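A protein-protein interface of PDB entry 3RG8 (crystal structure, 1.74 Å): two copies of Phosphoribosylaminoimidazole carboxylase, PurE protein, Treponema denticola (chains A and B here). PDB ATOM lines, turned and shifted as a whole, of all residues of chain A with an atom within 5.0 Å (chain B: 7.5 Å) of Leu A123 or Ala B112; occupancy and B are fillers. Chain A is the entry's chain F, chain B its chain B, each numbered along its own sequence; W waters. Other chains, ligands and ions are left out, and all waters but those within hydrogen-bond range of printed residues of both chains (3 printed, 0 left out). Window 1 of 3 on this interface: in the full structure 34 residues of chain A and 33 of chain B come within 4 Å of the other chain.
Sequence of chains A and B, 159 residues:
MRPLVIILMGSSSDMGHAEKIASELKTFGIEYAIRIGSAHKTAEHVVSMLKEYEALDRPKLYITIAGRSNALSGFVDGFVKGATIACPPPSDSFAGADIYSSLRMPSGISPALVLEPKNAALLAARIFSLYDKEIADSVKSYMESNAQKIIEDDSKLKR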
ATOM      1  N   ILE A  85     -34.651  -4.283  10.209  1.00  0.00           N
ATOM      2  CA  ILE A  85     -33.633  -3.559   9.482  1.00  0.00           C
ATOM      3  C   ILE A  85     -33.373  -2.235  10.164  1.00  0.00           C
ATOM      4  O   ILE A  85     -34.310  -1.488  10.437  1.00  0.00           O
ATOM      5  CB  ILE A  85     -34.120  -3.285   8.031  1.00  0.00           C
ATOM      6  CG1 ILE A  85     -34.432  -4.602   7.278  1.00  0.00           C
ATOM      7  CG2 ILE A  85     -33.096  -2.507   7.198  1.00  0.00           C
ATOM      8  CD1 ILE A  85     -35.225  -4.371   5.957  1.00  0.00           C
ATOM      9  N   ALA A 112     -30.583  -5.984  10.301  1.00  0.00           N
ATOM     10  CA  ALA A 112     -29.855  -5.745   9.051  1.00  0.00           C
ATOM     11  C   ALA A 112     -29.513  -4.257   8.953  1.00  0.00           C
ATOM     12  O   ALA A 112     -30.422  -3.386   8.905  1.00  0.00           O
ATOM     13  CB  ALA A 112     -30.675  -6.144   7.880  1.00  0.00           C
ATOM     14  N   LEU A 113     -28.226  -3.961   8.896  1.00  0.00           N
ATOM     15  CA  LEU A 113     -27.818  -2.577   8.724  1.00  0.00           C
ATOM     16  C   LEU A 113     -27.735  -2.249   7.232  1.00  0.00           C
ATOM     17  O   LEU A 113     -26.950  -2.902   6.481  1.00  0.00           O
ATOM     18  CB  LEU A 113     -26.505  -2.275   9.429  1.00  0.00           C
ATOM     19  CG  LEU A 113     -26.021  -0.837   9.430  1.00  0.00           C
ATOM     20  CD1 LEU A 113     -27.118   0.179   9.909  1.00  0.00           C
ATOM     21  CD2 LEU A 113     -24.643  -0.832  10.195  1.00  0.00           C
ATOM     22  N   VAL A 114     -28.471  -1.209   6.839  1.00  0.00           N
ATOM     23  CA  VAL A 114     -28.404  -0.662   5.477  1.00  0.00           C
ATOM     24  C   VAL A 114     -28.364   0.852   5.643  1.00  0.00           C
ATOM     25  O   VAL A 114     -29.217   1.408   6.359  1.00  0.00           O
ATOM     26  CB  VAL A 114     -29.636  -1.033   4.696  1.00  0.00           C
ATOM     27  CG1 VAL A 114     -29.764  -0.228   3.366  1.00  0.00           C
ATOM     28  CG2 VAL A 114     -29.673  -2.563   4.478  1.00  0.00           C
ATOM     29  N   ASN A 119     -32.403   1.872  -0.221  1.00  0.00           N
ATOM     30  CA  ASN A 119     -31.847   0.551  -0.093  1.00  0.00           C
ATOM     31  C   ASN A 119     -32.459  -0.257   1.066  1.00  0.00           C
ATOM     32  O   ASN A 119     -32.610  -1.463   0.978  1.00  0.00           O
ATOM     33  CB  ASN A 119     -30.307   0.584   0.040  1.00  0.00           C
ATOM     34  CG  ASN A 119     -29.610   0.983  -1.275  1.00  0.00           C
ATOM     35  OD1 ASN A 119     -30.193   0.912  -2.348  1.00  0.00           O
ATOM     36  ND2 ASN A 119     -28.357   1.482  -1.182  1.00  0.00           N
ATOM     37  N   ALA A 120     -32.865   0.434   2.121  1.00  0.00           N
ATOM     38  CA  ALA A 120     -33.627  -0.217   3.207  1.00  0.00           C
ATOM     39  C   ALA A 120     -34.938  -0.792   2.683  1.00  0.00           C
ATOM     40  O   ALA A 120     -35.280  -1.942   2.995  1.00  0.00           O
ATOM     41  CB  ALA A 120     -33.894   0.748   4.337  1.00  0.00           C
ATOM     42  N   ALA A 121     -35.666   0.001   1.884  1.00  0.00           N
ATOM     43  CA  ALA A 121     -36.944  -0.404   1.278  1.00  0.00           C
ATOM     44  C   ALA A 121     -36.647  -1.595   0.341  1.00  0.00           C
ATOM     45  O   ALA A 121     -37.410  -2.558   0.313  1.00  0.00           O
ATOM     46  CB  ALA A 121     -37.574   0.751   0.508  1.00  0.00           C
ATOM     47  N   LEU A 122     -35.558  -1.527  -0.436  1.00  0.00           N
ATOM     48  CA  LEU A 122     -35.272  -2.574  -1.412  1.00  0.00           C
ATOM     49  C   LEU A 122     -34.960  -3.894  -0.716  1.00  0.00           C
ATOM     50  O   LEU A 122     -35.455  -4.953  -1.137  1.00  0.00           O
ATOM     51  CB  LEU A 122     -34.106  -2.158  -2.321  1.00  0.00           C
ATOM     52  CG  LEU A 122     -33.648  -3.175  -3.369  1.00  0.00           C
ATOM     53  CD1 LEU A 122     -34.721  -3.483  -4.414  1.00  0.00           C
ATOM     54  CD2 LEU A 122     -32.337  -2.657  -3.981  1.00  0.00           C
ATOM     55  N   LEU A 123     -34.127  -3.816   0.314  1.00  0.00           N
ATOM     56  CA  LEU A 123     -33.837  -4.990   1.118  1.00  0.00           C
ATOM     57  C   LEU A 123     -35.142  -5.613   1.564  1.00  0.00           C
ATOM     58  O   LEU A 123     -35.330  -6.844   1.424  1.00  0.00           O
ATOM     59  CB  LEU A 123     -32.983  -4.672   2.329  1.00  0.00           C
ATOM     60  CG  LEU A 123     -32.725  -5.912   3.239  1.00  0.00           C
ATOM     61  CD1 LEU A 123     -32.190  -7.128   2.476  1.00  0.00           C
ATOM     62  CD2 LEU A 123     -31.802  -5.493   4.359  1.00  0.00           C
ATOM     63  N   ALA A 124     -36.021  -4.788   2.146  1.00  0.00           N
ATOM     64  CA  ALA A 124     -37.311  -5.280   2.631  1.00  0.00           C
ATOM     65  C   ALA A 124     -38.059  -6.034   1.565  1.00  0.00           C
ATOM     66  O   ALA A 124     -38.515  -7.166   1.767  1.00  0.00           O
ATOM     67  CB  ALA A 124     -38.176  -4.120   3.141  1.00  0.00           C
ATOM     68  N   ALA A 125     -38.234  -5.403   0.403  1.00  0.00           N
ATOM     69  CA  ALA A 125     -38.925  -6.038  -0.695  1.00  0.00           C
ATOM     70  C   ALA A 125     -38.286  -7.358  -1.045  1.00  0.00           C
ATOM     71  O   ALA A 125     -38.963  -8.364  -1.343  1.00  0.00           O
ATOM     72  CB  ALA A 125     -38.890  -5.130  -1.931  1.00  0.00           C
ATOM     73  N   ARG A 126     -36.968  -7.334  -1.092  1.00  0.00           N
ATOM     74  CA  ARG A 126     -36.209  -8.505  -1.461  1.00  0.00           C
ATOM     75  C   ARG A 126     -36.334  -9.618  -0.420  1.00  0.00           C
ATOM     76  O   ARG A 126     -36.315 -10.784  -0.796  1.00  0.00           O
ATOM     77  CB  ARG A 126     -34.762  -8.137  -1.794  1.00  0.00           C
ATOM     78  CG  ARG A 126     -34.660  -7.426  -3.112  1.00  0.00           C
ATOM     79  CD  ARG A 126     -33.275  -6.899  -3.325  1.00  0.00           C
ATOM     80  NE  ARG A 126     -32.374  -7.938  -3.845  1.00  0.00           N
ATOM     81  CZ  ARG A 126     -31.109  -7.698  -4.125  1.00  0.00           C
ATOM     82  NH1 ARG A 126     -30.621  -6.478  -3.924  1.00  0.00           N
ATOM     83  NH2 ARG A 126     -30.329  -8.651  -4.593  1.00  0.00           N
ATOM     84  N   ILE A 127     -36.570  -9.272   0.846  1.00  0.00           N
ATOM     85  CA  ILE A 127     -36.806 -10.256   1.878  1.00  0.00           C
ATOM     86  C   ILE A 127     -38.164 -10.931   1.566  1.00  0.00           C
ATOM     87  O   ILE A 127     -38.257 -12.166   1.526  1.00  0.00           O
ATOM     88  CB  ILE A 127     -36.794  -9.635   3.297  1.00  0.00           C
ATOM     89  CG1 ILE A 127     -35.323  -9.381   3.738  1.00  0.00           C
ATOM     90  CG2 ILE A 127     -37.501 -10.554   4.328  1.00  0.00           C
ATOM     91  CD1 ILE A 127     -35.102  -8.418   4.909  1.00  0.00           C
ATOM     92  N   LEU B  61     -31.135 -17.476   0.385  1.00  0.00           N
ATOM     93  CA  LEU B  61     -30.352 -16.298   0.731  1.00  0.00           C
ATOM     94  C   LEU B  61     -28.885 -16.535   0.382  1.00  0.00           C
ATOM     95  O   LEU B  61     -28.446 -17.672   0.268  1.00  0.00           O
ATOM     96  CB  LEU B  61     -30.521 -15.929   2.191  1.00  0.00           C
ATOM     97  CG  LEU B  61     -31.887 -15.415   2.575  1.00  0.00           C
ATOM     98  CD1 LEU B  61     -32.020 -15.452   4.115  1.00  0.00           C
ATOM     99  CD2 LEU B  61     -32.183 -14.056   2.049  1.00  0.00           C
ATOM    100  N   TYR B  62     -28.151 -15.454   0.167  1.00  0.00           N
ATOM    101  CA  TYR B  62     -26.708 -15.524  -0.046  1.00  0.00           C
ATOM    102  C   TYR B  62     -26.063 -14.765   1.090  1.00  0.00           C
ATOM    103  O   TYR B  62     -26.473 -13.647   1.368  1.00  0.00           O
ATOM    104  CB  TYR B  62     -26.292 -14.900  -1.396  1.00  0.00           C
ATOM    105  CG  TYR B  62     -26.841 -15.608  -2.604  1.00  0.00           C
ATOM    106  CD1 TYR B  62     -28.159 -15.358  -3.030  1.00  0.00           C
ATOM    107  CD2 TYR B  62     -26.087 -16.534  -3.326  1.00  0.00           C
ATOM    108  CE1 TYR B  62     -28.706 -15.994  -4.119  1.00  0.00           C
ATOM    109  CE2 TYR B  62     -26.639 -17.196  -4.422  1.00  0.00           C
ATOM    110  CZ  TYR B  62     -27.943 -16.904  -4.831  1.00  0.00           C
ATOM    111  OH  TYR B  62     -28.538 -17.522  -5.913  1.00  0.00           O
ATOM    112  N   ILE B  63     -25.119 -15.388   1.809  1.00  0.00           N
ATOM    113  CA  ILE B  63     -24.308 -14.704   2.793  1.00  0.00           C
ATOM    114  C   ILE B  63     -22.897 -14.652   2.201  1.00  0.00           C
ATOM    115  O   ILE B  63     -22.280 -15.676   1.909  1.00  0.00           O
ATOM    116  CB  ILE B  63     -24.275 -15.359   4.182  1.00  0.00           C
ATOM    117  CG1 ILE B  63     -25.692 -15.355   4.785  1.00  0.00           C
ATOM    118  CG2 ILE B  63     -23.377 -14.610   5.083  1.00  0.00           C
ATOM    119  CD1 ILE B  63     -25.853 -16.201   6.015  1.00  0.00           C
ATOM    120  N   THR B  64     -22.411 -13.435   2.035  1.00  0.00           N
ATOM    121  CA  THR B  64     -21.208 -13.183   1.304  1.00  0.00           C
ATOM    122  C   THR B  64     -20.119 -12.674   2.233  1.00  0.00           C
ATOM    123  O   THR B  64     -20.333 -11.705   2.959  1.00  0.00           O
ATOM    124  CB  THR B  64     -21.497 -12.147   0.140  1.00  0.00           C
ATOM    125  OG1 THR B  64     -22.207 -10.978   0.655  1.00  0.00           O
ATOM    126  CG2 THR B  64     -22.227 -12.852  -1.022  1.00  0.00           C
ATOM    127  N   SER B  73     -19.671  -8.721  -1.830  1.00  0.00           N
ATOM    128  CA  SER B  73     -21.068  -8.616  -1.380  1.00  0.00           C
ATOM    129  C   SER B  73     -21.952  -7.805  -2.371  1.00  0.00           C
ATOM    130  O   SER B  73     -23.092  -8.199  -2.717  1.00  0.00           O
ATOM    131  CB  SER B  73     -21.125  -8.060   0.026  1.00  0.00           C
ATOM    132  OG  SER B  73     -20.589  -8.957   0.991  1.00  0.00           O
ATOM    133  N   ASP B  77     -24.961  -9.203  -4.744  1.00  0.00           N
ATOM    134  CA  ASP B  77     -26.259  -8.585  -4.466  1.00  0.00           C
ATOM    135  C   ASP B  77     -26.841  -7.967  -5.758  1.00  0.00           C
ATOM    136  O   ASP B  77     -28.040  -8.046  -6.003  1.00  0.00           O
ATOM    137  CB  ASP B  77     -26.132  -7.496  -3.414  1.00  0.00           C
ATOM    138  CG  ASP B  77     -27.482  -7.022  -2.936  1.00  0.00           C
ATOM    139  OD1 ASP B  77     -28.113  -7.684  -2.054  1.00  0.00           O
ATOM    140  OD2 ASP B  77     -27.943  -5.996  -3.474  1.00  0.00           O
ATOM    141  N   GLY B  82     -33.085 -12.129  -5.077  1.00  0.00           N
ATOM    142  CA  GLY B  82     -33.471 -12.127  -3.692  1.00  0.00           C
ATOM    143  C   GLY B  82     -32.480 -11.431  -2.775  1.00  0.00           C
ATOM    144  O   GLY B  82     -31.382 -11.017  -3.222  1.00  0.00           O
ATOM    145  N   ALA B  83     -32.838 -11.349  -1.480  1.00  0.00           N
ATOM    146  CA  ALA B  83     -32.013 -10.636  -0.496  1.00  0.00           C
ATOM    147  C   ALA B  83     -30.664 -11.330  -0.255  1.00  0.00           C
ATOM    148  O   ALA B  83     -30.514 -12.542  -0.431  1.00  0.00           O
ATOM    149  CB  ALA B  83     -32.761 -10.492   0.801  1.00  0.00           C
ATOM    150  N   THR B  84     -29.652 -10.542   0.104  1.00  0.00           N
ATOM    151  CA  THR B  84     -28.367 -11.079   0.466  1.00  0.00           C
ATOM    152  C   THR B  84     -27.906 -10.434   1.795  1.00  0.00           C
ATOM    153  O   THR B  84     -28.456  -9.425   2.255  1.00  0.00           O
ATOM    154  CB  THR B  84     -27.301 -10.843  -0.642  1.00  0.00           C
ATOM    155  OG1 THR B  84     -26.868  -9.482  -0.624  1.00  0.00           O
ATOM    156  CG2 THR B  84     -27.886 -11.198  -2.022  1.00  0.00           C
ATOM    157  N   ILE B  85     -26.940 -11.085   2.427  1.00  0.00           N
ATOM    158  CA  ILE B  85     -26.353 -10.662   3.640  1.00  0.00           C
ATOM    159  C   ILE B  85     -24.824 -10.571   3.528  1.00  0.00           C
ATOM    160  O   ILE B  85     -24.162 -11.502   3.113  1.00  0.00           O
ATOM    161  CB  ILE B  85     -26.730 -11.649   4.810  1.00  0.00           C
ATOM    162  CG1 ILE B  85     -28.244 -11.684   5.085  1.00  0.00           C
ATOM    163  CG2 ILE B  85     -26.021 -11.243   6.024  1.00  0.00           C
ATOM    164  CD1 ILE B  85     -28.713 -12.896   5.979  1.00  0.00           C
ATOM    165  N   ALA B  86     -24.276  -9.429   3.921  1.00  0.00           N
ATOM    166  CA  ALA B  86     -22.832  -9.256   3.964  1.00  0.00           C
ATOM    167  C   ALA B  86     -22.344  -9.531   5.378  1.00  0.00           C
ATOM    168  O   ALA B  86     -22.822  -8.909   6.347  1.00  0.00           O
ATOM    169  CB  ALA B  86     -22.486  -7.838   3.533  1.00  0.00           C
ATOM    170  N   CYS B  87     -21.386 -10.466   5.511  1.00  0.00           N
ATOM    171  CA  CYS B  87     -20.793 -10.732   6.818  1.00  0.00           C
ATOM    172  C   CYS B  87     -19.285 -10.874   6.641  1.00  0.00           C
ATOM    173  O   CYS B  87     -18.760 -11.977   6.424  1.00  0.00           O
ATOM    174  CB  CYS B  87     -21.405 -11.911   7.502  1.00  0.00           C
ATOM    175  SG  CYS B  87     -20.786 -12.228   9.110  1.00  0.00           S
ATOM    176  N   PRO B  88     -18.598  -9.719   6.659  1.00  0.00           N
ATOM    177  CA  PRO B  88     -17.137  -9.737   6.474  1.00  0.00           C
ATOM    178  C   PRO B  88     -16.430 -10.345   7.628  1.00  0.00           C
ATOM    179  O   PRO B  88     -16.923 -10.278   8.754  1.00  0.00           O
ATOM    180  CB  PRO B  88     -16.747  -8.237   6.378  1.00  0.00           C
ATOM    181  CG  PRO B  88     -17.818  -7.500   7.055  1.00  0.00           C
ATOM    182  CD  PRO B  88     -19.105  -8.359   6.833  1.00  0.00           C
ATOM    183  N   SER B 102     -17.932  -2.544   3.028  1.00  0.00           N
ATOM    184  CA  SER B 102     -19.242  -3.232   3.120  1.00  0.00           C
ATOM    185  C   SER B 102     -20.479  -2.335   3.333  1.00  0.00           C
ATOM    186  O   SER B 102     -21.613  -2.737   2.959  1.00  0.00           O
ATOM    187  CB  SER B 102     -19.205  -4.230   4.264  1.00  0.00           C
ATOM    188  OG  SER B 102     -18.344  -5.289   3.946  1.00  0.00           O
ATOM    189  N   ILE B 109     -28.393  -1.265  -4.507  1.00  0.00           N
ATOM    190  CA  ILE B 109     -27.597  -2.441  -4.102  1.00  0.00           C
ATOM    191  C   ILE B 109     -27.810  -2.558  -2.604  1.00  0.00           C
ATOM    192  O   ILE B 109     -27.445  -1.629  -1.876  1.00  0.00           O
ATOM    193  CB  ILE B 109     -26.114  -2.260  -4.432  1.00  0.00           C
ATOM    194  CG1 ILE B 109     -25.928  -2.216  -5.935  1.00  0.00           C
ATOM    195  CG2 ILE B 109     -25.230  -3.322  -3.708  1.00  0.00           C
ATOM    196  CD1 ILE B 109     -26.133  -3.538  -6.640  1.00  0.00           C
ATOM    197  N   SER B 110     -28.415  -3.646  -2.123  1.00  0.00           N
ATOM    198  CA  SER B 110     -28.984  -3.629  -0.768  1.00  0.00           C
ATOM    199  C   SER B 110     -28.631  -4.833   0.121  1.00  0.00           C
ATOM    200  O   SER B 110     -29.534  -5.423   0.744  1.00  0.00           O
ATOM    201  CB  SER B 110     -30.507  -3.466  -0.816  1.00  0.00           C
ATOM    202  OG  SER B 110     -31.107  -4.589  -1.415  1.00  0.00           O
ATOM    203  N   PRO B 111     -27.367  -5.230   0.140  1.00  0.00           N
ATOM    204  CA  PRO B 111     -27.067  -6.326   1.087  1.00  0.00           C
ATOM    205  C   PRO B 111     -27.247  -5.850   2.502  1.00  0.00           C
ATOM    206  O   PRO B 111     -26.905  -4.697   2.840  1.00  0.00           O
ATOM    207  CB  PRO B 111     -25.615  -6.617   0.801  1.00  0.00           C
ATOM    208  CG  PRO B 111     -25.079  -5.271   0.369  1.00  0.00           C
ATOM    209  CD  PRO B 111     -26.119  -4.731  -0.489  1.00  0.00           C
ATOM    210  N   ALA B 112     -27.751  -6.752   3.332  1.00  0.00           N
ATOM    211  CA  ALA B 112     -27.873  -6.560   4.763  1.00  0.00           C
ATOM    212  C   ALA B 112     -26.519  -6.777   5.451  1.00  0.00           C
ATOM    213  O   ALA B 112     -25.963  -7.870   5.420  1.00  0.00           O
ATOM    214  CB  ALA B 112     -28.932  -7.565   5.309  1.00  0.00           C
ATOM    215  N   LEU B 113     -25.988  -5.755   6.103  1.00  0.00           N
ATOM    216  CA  LEU B 113     -24.687  -5.872   6.740  1.00  0.00           C
ATOM    217  C   LEU B 113     -24.912  -6.354   8.194  1.00  0.00           C
ATOM    218  O   LEU B 113     -25.654  -5.727   8.934  1.00  0.00           O
ATOM    219  CB  LEU B 113     -23.931  -4.530   6.753  1.00  0.00           C
ATOM    220  CG  LEU B 113     -22.499  -4.550   7.315  1.00  0.00           C
ATOM    221  CD1 LEU B 113     -21.670  -5.748   6.695  1.00  0.00           C
ATOM    222  CD2 LEU B 113     -21.757  -3.201   7.158  1.00  0.00           C
ATOM    223  N   VAL B 114     -24.275  -7.436   8.573  1.00  0.00           N
ATOM    224  CA  VAL B 114     -24.217  -7.875   9.985  1.00  0.00           C
ATOM    225  C   VAL B 114     -22.775  -8.274  10.308  1.00  0.00           C
ATOM    226  O   VAL B 114     -22.159  -9.033   9.539  1.00  0.00           O
ATOM    227  CB  VAL B 114     -25.196  -9.050  10.191  1.00  0.00           C
ATOM    228  CG1 VAL B 114     -25.097  -9.719  11.598  1.00  0.00           C
ATOM    229  CG2 VAL B 114     -26.564  -8.622   9.961  1.00  0.00           C
ATOM    230  N   LEU B 115     -22.213  -7.800  11.435  1.00  0.00           N
ATOM    231  CA  LEU B 115     -20.826  -8.076  11.770  1.00  0.00           C
ATOM    232  C   LEU B 115     -20.549  -9.541  12.178  1.00  0.00           C
ATOM    233  O   LEU B 115     -19.564 -10.128  11.709  1.00  0.00           O
ATOM    234  CB  LEU B 115     -20.318  -7.107  12.876  1.00  0.00           C
ATOM    235  CG  LEU B 115     -20.163  -5.640  12.461  1.00  0.00           C
ATOM    236  CD1 LEU B 115     -19.581  -4.876  13.640  1.00  0.00           C
ATOM    237  CD2 LEU B 115     -19.221  -5.529  11.248  1.00  0.00           C
ATOM    238  N   ALA B 120     -25.284 -13.196  11.676  1.00  0.00           N
ATOM    239  CA  ALA B 120     -25.600 -13.280  10.236  1.00  0.00           C
ATOM    240  C   ALA B 120     -26.536 -14.509  10.015  1.00  0.00           C
ATOM    241  O   ALA B 120     -27.545 -14.425   9.331  1.00  0.00           O
ATOM    242  CB  ALA B 120     -24.314 -13.401   9.391  1.00  0.00           C
ATOM    243  N   LEU B 123     -29.946 -13.632  11.479  1.00  0.00           N
ATOM    244  CA  LEU B 123     -30.700 -12.806  10.534  1.00  0.00           C
ATOM    245  C   LEU B 123     -31.319 -13.637   9.406  1.00  0.00           C
ATOM    246  O   LEU B 123     -32.508 -13.425   9.063  1.00  0.00           O
ATOM    247  CB  LEU B 123     -29.873 -11.667   9.952  1.00  0.00           C
ATOM    248  CG  LEU B 123     -30.563 -10.817   8.896  1.00  0.00           C
ATOM    249  CD1 LEU B 123     -31.794 -10.068   9.518  1.00  0.00           C
ATOM    250  CD2 LEU B 123     -29.526  -9.844   8.193  1.00  0.00           C
ATOM    251  N   ILE B 127     -35.217 -14.012   8.585  1.00  0.00           N
ATOM    252  CA  ILE B 127     -35.729 -13.734   7.284  1.00  0.00           C
ATOM    253  C   ILE B 127     -36.706 -14.841   6.796  1.00  0.00           C
ATOM    254  O   ILE B 127     -37.868 -14.545   6.416  1.00  0.00           O
ATOM    255  CB  ILE B 127     -34.589 -13.498   6.280  1.00  0.00           C
ATOM    256  CG1 ILE B 127     -34.029 -12.087   6.519  1.00  0.00           C
ATOM    257  CG2 ILE B 127     -35.090 -13.636   4.836  1.00  0.00           C
ATOM    258  CD1 ILE B 127     -32.792 -11.772   5.711  1.00  0.00           C
HETATM  259  O   HOH W   1     -27.143  -0.767   0.846  1.00  0.00           O
HETATM  260  O   HOH W   2     -25.854  -2.831   4.186  1.00  0.00           O
HETATM  261  O   HOH W   3     -38.974 -14.063   3.671  1.00  0.00           O
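The side-chain carboxylate of Asp B77 is in salt-bridge range of the guanidinium group of Arg A126 (2.8 Å). The backbone carbonyl oxygen (O) of Gly B82 lies within hydrogen-bond range of the guanidinium group (NH2) of Arg A126, 2.9 Å away. O of Ile B109 is in hydrogen-bond range of ND2 of Asn A119, at 3.3 Å. The guanidinium group of Arg A126 is in hydrogen-bond range of the side-chain hydroxyl of Ser B110 (3.2 Å). The backbone NH of Leu B113 sits at hydrogen-bond distance from the backbone carbonyl oxygen of Leu A113.
OG1 of Thr B84 lies within hydrogen-bond range of OD1 of Asp B77, at 2.6 Å. The side-chain carboxylate of Asp B77 lies within hydrogen-bond range of the backbone NH of Ser B110 (2.8 Å). The backbone carbonyl oxygen (O) of Thr B84 sits at hydrogen-bond distance from the backbone NH (N) of Ala B112 (3.0 Å). N of Ala B86 sits at hydrogen-bond distance from O of Ala B112 (2.7 Å).
Among the printed residues, merely in contact across the chains: Asn A119 with Ser B110, Ala A112 with Ala B112, Leu A122 with Ser B110, Leu A123 with Ser B110, Arg A126 with Ala B83, Leu A123 with Ala B112, Leu A123 with Ala B83, Val A114 with Pro B111, Ala A112 with Leu B123, Ile A127 with Ile B127 and Ile A127 with Ala B83.
Of chain B, only Ala B83, Ser B110 and Ala B112 come within 4 Å of Leu A123. Of the printed residues of chain B, Ile A127 touches Ala B83 and Ile B127. Leu B61 touches none of the printed residues of chain A. Of the printed residues of chain A, Ala B83 touches Leu A123, Arg A126 and Ile A127. Printed residues of chain A within 4 Å of Ala B112: Ala A112 and Leu A123. Ala B120 touches none of the printed residues of chain A. The nearest residue of chain B that does not touch Leu A123 is Thr B84 (4.4 Å). The nearest residue of chain A that does not touch Ala B112 is Leu A113 (4.03 Å). The nearest printed residue of chain A that does not touch Ile B127 is Leu A123 (5.7 Å).
Printed residues of chain A that touch a printed residue of chain B: Ala A112, Leu A113, Val A114, Asn A119, Leu A122, Leu A123, Arg A126 and Ile A127. Hydrophobic or aromatic side chains of chain A that line the printed part of chain B: Ala A112, Leu A113, Val A114, Leu A122, Leu A123 and Ile A127. Printed residues of chain B that touch a printed residue of chain A: Asp B77, Gly B82, Ala B83, Ile B109, Ser B110, Pro B111, Ala B112, Leu B113, Leu B123 and Ile B127. Hydrophobic or aromatic side chains of chain B within 4 Å of the printed part of chain A: Ala B83, Ala B112, Leu B113, Leu B123 and Ile B127. Among the printed residues, 16 pairs touch across the chains. Among the printed residues, Asp or Glu carboxylates within 4 Å of a Lys or Arg side-chain nitrogen of the other chain: Arg A126 with Asp B77 (2.8 Å).
Ala A112 touches its own counterpart, Ala B112. Ala A112 touches Leu B123, and with the chains exchanged Leu A123 touches Ala B112. Leu A113 touches its own counterpart, Leu B113. Ile A127 touches its own counterpart, Ile B127. Positions printed for both chains: 85, 112, 113, 114, 120, 123 and 127.
Water W2 lies within hydrogen-bond range of the backbone carbonyl oxygen (O) of Pro B111, the backbone carbonyl oxygen (O) of Leu A113 and the backbone NH (N) of Leu B113. Water W1 bridges the backbone carbonyl oxygen (O) of Ile B109 (2.9 Å) and the side-chain amide nitrogen (ND2) of Asn A119 (3.3 Å). Water W3 lies within hydrogen-bond range of the backbone carbonyl oxygen of Ile A127 and the backbone carbonyl oxygen of Ile B127.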
